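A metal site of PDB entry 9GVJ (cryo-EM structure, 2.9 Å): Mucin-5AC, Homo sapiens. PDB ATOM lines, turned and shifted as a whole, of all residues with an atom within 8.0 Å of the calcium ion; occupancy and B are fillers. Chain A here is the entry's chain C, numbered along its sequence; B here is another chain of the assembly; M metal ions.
N of Asp 888 lies close to OG1 of Thr 886 (3.5 Å). The backbone NH (N) of Gly 1003 is in hydrogen-bond range of the backbone carbonyl oxygen (O) of Asn 1011, 3.3 Å away. N of Asp 1014 sits at hydrogen-bond distance from OD1 of Asp 888 (2.8 Å). OD2 of Asp 1019 lies within hydrogen-bond range of OG1 of Thr 886 (2.5 Å).
Six residues have an atom within 4 Å of the calcium ion: Asp 888, Asn 1011, Asp 1013, Ile 1015, Asn 1018 and Asp 1019. The nearest printed residue that does not touch the calcium ion is Ala 1016 (4.5 Å).
OD1 of Asp 1019 is bound to the calcium ion. The calcium ion is bound by O of Ile 1015. OD1 of Asp 1013 binds the calcium ion, at 2.2 Å. The side-chain amide oxygen (OD1) of Asn 1018 binds the calcium ion, 2.2 Å away. The calcium ion is bound by the side-chain amide oxygen (OD1) of Asn 1011, 2.3 Å away. The calcium ion is bound by the side-chain carboxylate (OD2) of Asp 888, 2.6 Å away.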
ATOM      1  N   THR A 886       3.894  12.665 -12.994  1.00  0.00           N
ATOM      2  CA  THR A 886       3.021  13.835 -12.999  1.00  0.00           C
ATOM      3  C   THR A 886       1.910  13.685 -11.967  1.00  0.00           C
ATOM      4  O   THR A 886       1.809  12.691 -11.243  1.00  0.00           O
ATOM      5  CB  THR A 886       2.443  14.050 -14.394  1.00  0.00           C
ATOM      6  OG1 THR A 886       1.487  13.020 -14.685  1.00  0.00           O
ATOM      7  CG2 THR A 886       3.555  14.008 -15.445  1.00  0.00           C
ATOM      8  N   PHE A 887       1.045  14.709 -11.901  1.00  0.00           N
ATOM      9  CA  PHE A 887      -0.091  14.673 -10.983  1.00  0.00           C
ATOM     10  C   PHE A 887      -1.043  13.544 -11.328  1.00  0.00           C
ATOM     11  O   PHE A 887      -1.595  12.882 -10.443  1.00  0.00           O
ATOM     12  CB  PHE A 887      -0.826  16.015 -11.000  1.00  0.00           C
ATOM     13  CG  PHE A 887      -0.046  17.144 -10.397  1.00  0.00           C
ATOM     14  CD1 PHE A 887       0.176  17.198  -9.026  1.00  0.00           C
ATOM     15  CD2 PHE A 887       0.442  18.166 -11.186  1.00  0.00           C
ATOM     16  CE1 PHE A 887       0.884  18.243  -8.476  1.00  0.00           C
ATOM     17  CE2 PHE A 887       1.151  19.211 -10.636  1.00  0.00           C
ATOM     18  CZ  PHE A 887       1.373  19.247  -9.277  1.00  0.00           C
ATOM     19  N   ASP A 888      -1.264  13.304 -12.617  1.00  0.00           N
ATOM     20  CA  ASP A 888      -2.227  12.314 -13.087  1.00  0.00           C
ATOM     21  C   ASP A 888      -1.640  10.920 -13.196  1.00  0.00           C
ATOM     22  O   ASP A 888      -2.335   9.999 -13.641  1.00  0.00           O
ATOM     23  CB  ASP A 888      -2.809  12.745 -14.435  1.00  0.00           C
ATOM     24  CG  ASP A 888      -3.629  14.017 -14.334  1.00  0.00           C
ATOM     25  OD1 ASP A 888      -4.135  14.311 -13.232  1.00  0.00           O
ATOM     26  OD2 ASP A 888      -3.750  14.723 -15.351  1.00  0.00           O
ATOM     27  N   GLY A 889      -0.384  10.734 -12.808  1.00  0.00           N
ATOM     28  CA  GLY A 889       0.234   9.420 -12.795  1.00  0.00           C
ATOM     29  C   GLY A 889       1.042   9.072 -14.023  1.00  0.00           C
ATOM     30  O   GLY A 889       1.389   7.886 -14.185  1.00  0.00           O
ATOM     31  N   GLN A 890       1.354  10.030 -14.890  1.00  0.00           N
ATOM     32  CA  GLN A 890       2.159   9.761 -16.076  1.00  0.00           C
ATOM     33  C   GLN A 890       3.629   9.747 -15.680  1.00  0.00           C
ATOM     34  O   GLN A 890       4.170  10.769 -15.245  1.00  0.00           O
ATOM     35  CB  GLN A 890       1.887  10.799 -17.156  1.00  0.00           C
ATOM     36  CG  GLN A 890       2.789  10.693 -18.364  1.00  0.00           C
ATOM     37  CD  GLN A 890       2.464   9.488 -19.226  1.00  0.00           C
ATOM     38  OE1 GLN A 890       1.351   9.345 -19.731  1.00  0.00           O
ATOM     39  NE2 GLN A 890       3.445   8.608 -19.416  1.00  0.00           N
ATOM     40  N   GLY A1003      -7.134  21.003 -13.439  1.00  0.00           N
ATOM     41  CA  GLY A1003      -7.366  21.565 -14.748  1.00  0.00           C
ATOM     42  C   GLY A1003      -6.892  22.987 -14.923  1.00  0.00           C
ATOM     43  O   GLY A1003      -7.169  23.589 -15.965  1.00  0.00           O
ATOM     44  N   VAL A1005      -3.477  24.003 -14.217  1.00  0.00           N
ATOM     45  CA  VAL A1005      -2.017  24.015 -14.131  1.00  0.00           C
ATOM     46  C   VAL A1005      -1.439  23.426 -15.410  1.00  0.00           C
ATOM     47  O   VAL A1005      -2.126  22.780 -16.198  1.00  0.00           O
ATOM     48  CB  VAL A1005      -1.500  23.242 -12.902  1.00  0.00           C
ATOM     49  CG1 VAL A1005      -1.794  24.017 -11.620  1.00  0.00           C
ATOM     50  CG2 VAL A1005      -2.131  21.863 -12.836  1.00  0.00           C
ATOM     51  N   CYS A1009       4.774  18.786 -15.030  1.00  0.00           N
ATOM     52  CA  CYS A1009       4.037  17.970 -14.074  1.00  0.00           C
ATOM     53  C   CYS A1009       2.621  17.664 -14.538  1.00  0.00           C
ATOM     54  O   CYS A1009       1.813  17.161 -13.760  1.00  0.00           O
ATOM     55  CB  CYS A1009       3.989  18.669 -12.713  1.00  0.00           C
ATOM     56  SG  CYS A1009       5.434  18.386 -11.672  1.00  0.00           S
ATOM     57  N   GLY A1010       2.300  17.943 -15.798  1.00  0.00           N
ATOM     58  CA  GLY A1010       0.965  17.706 -16.307  1.00  0.00           C
ATOM     59  C   GLY A1010       0.010  18.832 -15.993  1.00  0.00           C
ATOM     60  O   GLY A1010       0.394  19.923 -15.552  1.00  0.00           O
ATOM     61  N   ASN A1011      -1.265  18.564 -16.230  1.00  0.00           N
ATOM     62  CA  ASN A1011      -2.321  19.557 -16.058  1.00  0.00           C
ATOM     63  C   ASN A1011      -3.350  19.196 -15.001  1.00  0.00           C
ATOM     64  O   ASN A1011      -4.286  19.976 -14.790  1.00  0.00           O
ATOM     65  CB  ASN A1011      -3.028  19.820 -17.393  1.00  0.00           C
ATOM     66  CG  ASN A1011      -3.969  18.708 -17.778  1.00  0.00           C
ATOM     67  OD1 ASN A1011      -3.605  17.530 -17.743  1.00  0.00           O
ATOM     68  ND2 ASN A1011      -5.185  19.059 -18.162  1.00  0.00           N
ATOM     69  N   PHE A1012      -3.206  18.051 -14.333  1.00  0.00           N
ATOM     70  CA  PHE A1012      -4.040  17.688 -13.186  1.00  0.00           C
ATOM     71  C   PHE A1012      -5.523  17.653 -13.551  1.00  0.00           C
ATOM     72  O   PHE A1012      -6.331  18.441 -13.069  1.00  0.00           O
ATOM     73  CB  PHE A1012      -3.784  18.643 -12.013  1.00  0.00           C
ATOM     74  CG  PHE A1012      -4.312  18.152 -10.686  1.00  0.00           C
ATOM     75  CD1 PHE A1012      -4.792  16.864 -10.543  1.00  0.00           C
ATOM     76  CD2 PHE A1012      -4.326  18.994  -9.592  1.00  0.00           C
ATOM     77  CE1 PHE A1012      -5.273  16.424  -9.328  1.00  0.00           C
ATOM     78  CE2 PHE A1012      -4.812  18.564  -8.369  1.00  0.00           C
ATOM     79  CZ  PHE A1012      -5.289  17.271  -8.242  1.00  0.00           C
ATOM     80  N   ASP A1013      -5.867  16.708 -14.430  1.00  0.00           N
ATOM     81  CA  ASP A1013      -7.266  16.484 -14.807  1.00  0.00           C
ATOM     82  C   ASP A1013      -7.595  14.988 -14.823  1.00  0.00           C
ATOM     83  O   ASP A1013      -8.501  14.560 -15.540  1.00  0.00           O
ATOM     84  CB  ASP A1013      -7.585  17.117 -16.160  1.00  0.00           C
ATOM     85  CG  ASP A1013      -6.832  16.474 -17.305  1.00  0.00           C
ATOM     86  OD1 ASP A1013      -5.772  15.857 -17.042  1.00  0.00           O
ATOM     87  OD2 ASP A1013      -7.287  16.577 -18.460  1.00  0.00           O
ATOM     88  N   ASP A1014      -6.850  14.198 -14.058  1.00  0.00           N
ATOM     89  CA  ASP A1014      -7.028  12.756 -13.862  1.00  0.00           C
ATOM     90  C   ASP A1014      -6.712  11.940 -15.115  1.00  0.00           C
ATOM     91  O   ASP A1014      -6.822  10.711 -15.072  1.00  0.00           O
ATOM     92  CB  ASP A1014      -8.449  12.401 -13.391  1.00  0.00           C
ATOM     93  CG  ASP A1014      -8.676  12.750 -11.933  1.00  0.00           C
ATOM     94  OD1 ASP A1014      -7.725  13.227 -11.278  1.00  0.00           O
ATOM     95  OD2 ASP A1014      -9.803  12.555 -11.442  1.00  0.00           O
ATOM     96  N   ILE A1015      -6.328  12.573 -16.216  1.00  0.00           N
ATOM     97  CA  ILE A1015      -5.982  11.875 -17.458  1.00  0.00           C
ATOM     98  C   ILE A1015      -4.476  11.978 -17.651  1.00  0.00           C
ATOM     99  O   ILE A1015      -3.900  13.075 -17.588  1.00  0.00           O
ATOM    100  CB  ILE A1015      -6.734  12.468 -18.659  1.00  0.00           C
ATOM    101  CG1 ILE A1015      -8.240  12.451 -18.395  1.00  0.00           C
ATOM    102  CG2 ILE A1015      -6.417  11.689 -19.911  1.00  0.00           C
ATOM    103  CD1 ILE A1015      -9.041  13.255 -19.384  1.00  0.00           C
ATOM    104  N   ALA A1016      -3.830  10.836 -17.884  1.00  0.00           N
ATOM    105  CA  ALA A1016      -2.377  10.789 -17.959  1.00  0.00           C
ATOM    106  C   ALA A1016      -1.838  10.898 -19.384  1.00  0.00           C
ATOM    107  O   ALA A1016      -0.714  11.373 -19.577  1.00  0.00           O
ATOM    108  CB  ALA A1016      -1.848   9.504 -17.321  1.00  0.00           C
ATOM    109  N   VAL A1017      -2.616  10.471 -20.386  1.00  0.00           N
ATOM    110  CA  VAL A1017      -2.112  10.467 -21.757  1.00  0.00           C
ATOM    111  C   VAL A1017      -1.920  11.895 -22.259  1.00  0.00           C
ATOM    112  O   VAL A1017      -0.975  12.179 -23.005  1.00  0.00           O
ATOM    113  CB  VAL A1017      -3.038   9.652 -22.668  1.00  0.00           C
ATOM    114  CG1 VAL A1017      -2.918   8.173 -22.354  1.00  0.00           C
ATOM    115  CG2 VAL A1017      -4.483  10.112 -22.526  1.00  0.00           C
ATOM    116  N   ASN A1018      -2.811  12.810 -21.880  1.00  0.00           N
ATOM    117  CA  ASN A1018      -2.724  14.190 -22.330  1.00  0.00           C
ATOM    118  C   ASN A1018      -1.786  15.041 -21.495  1.00  0.00           C
ATOM    119  O   ASN A1018      -1.711  16.249 -21.715  1.00  0.00           O
ATOM    120  CB  ASN A1018      -4.122  14.824 -22.363  1.00  0.00           C
ATOM    121  CG  ASN A1018      -4.800  14.826 -21.003  1.00  0.00           C
ATOM    122  OD1 ASN A1018      -4.178  14.566 -19.978  1.00  0.00           O
ATOM    123  ND2 ASN A1018      -6.088  15.137 -20.994  1.00  0.00           N
ATOM    124  N   ASP A1019      -1.066  14.447 -20.532  1.00  0.00           N
ATOM    125  CA  ASP A1019      -0.102  15.202 -19.755  1.00  0.00           C
ATOM    126  C   ASP A1019       1.101  15.632 -20.582  1.00  0.00           C
ATOM    127  O   ASP A1019       1.834  16.537 -20.168  1.00  0.00           O
ATOM    128  CB  ASP A1019       0.354  14.392 -18.537  1.00  0.00           C
ATOM    129  CG  ASP A1019      -0.553  14.571 -17.340  1.00  0.00           C
ATOM    130  OD1 ASP A1019      -1.601  15.237 -17.475  1.00  0.00           O
ATOM    131  OD2 ASP A1019      -0.216  14.043 -16.262  1.00  0.00           O
ATOM    132  N   PHE A1020       1.328  14.991 -21.721  1.00  0.00           N
ATOM    133  CA  PHE A1020       2.418  15.389 -22.607  1.00  0.00           C
ATOM    134  C   PHE A1020       1.986  16.538 -23.504  1.00  0.00           C
ATOM    135  O   PHE A1020       2.105  16.469 -24.726  1.00  0.00           O
ATOM    136  CB  PHE A1020       2.881  14.210 -23.462  1.00  0.00           C
ATOM    137  CG  PHE A1020       3.761  13.237 -22.726  1.00  0.00           C
ATOM    138  CD1 PHE A1020       4.224  13.523 -21.459  1.00  0.00           C
ATOM    139  CD2 PHE A1020       4.127  12.039 -23.316  1.00  0.00           C
ATOM    140  CE1 PHE A1020       5.027  12.637 -20.782  1.00  0.00           C
ATOM    141  CE2 PHE A1020       4.935  11.143 -22.648  1.00  0.00           C
ATOM    142  CZ  PHE A1020       5.391  11.445 -21.380  1.00  0.00           C
ATOM    143  N   ALA A1021       1.478  17.611 -22.894  1.00  0.00           N
ATOM    144  CA  ALA A1021       1.026  18.790 -23.620  1.00  0.00           C
ATOM    145  C   ALA A1021       2.143  19.821 -23.645  1.00  0.00           C
ATOM    146  O   ALA A1021       2.606  20.267 -22.600  1.00  0.00           O
ATOM    147  CB  ALA A1021      -0.236  19.380 -22.977  1.00  0.00           C
ATOM    148  N   VAL A1027      -0.913  18.075 -27.416  1.00  0.00           N
ATOM    149  CA  VAL A1027      -0.396  16.829 -26.859  1.00  0.00           C
ATOM    150  C   VAL A1027       0.410  16.101 -27.925  1.00  0.00           C
ATOM    151  O   VAL A1027      -0.088  15.845 -29.030  1.00  0.00           O
ATOM    152  CB  VAL A1027      -1.544  15.949 -26.322  1.00  0.00           C
ATOM    153  CG1 VAL A1027      -1.022  14.579 -25.935  1.00  0.00           C
ATOM    154  CG2 VAL A1027      -2.219  16.623 -25.149  1.00  0.00           C
ATOM    155  N   SER B 549     -10.943   6.834 -20.254  1.00  0.00           N
ATOM    156  CA  SER B 549      -9.786   7.681 -20.557  1.00  0.00           C
ATOM    157  C   SER B 549      -8.902   7.947 -19.345  1.00  0.00           C
ATOM    158  O   SER B 549      -8.008   8.797 -19.420  1.00  0.00           O
ATOM    159  CB  SER B 549     -10.219   9.011 -21.187  1.00  0.00           C
ATOM    160  OG  SER B 549     -10.814   8.810 -22.454  1.00  0.00           O
HETATM  161 CA    CA M   1      -3.777  15.289 -17.890  1.00  0.00          CA
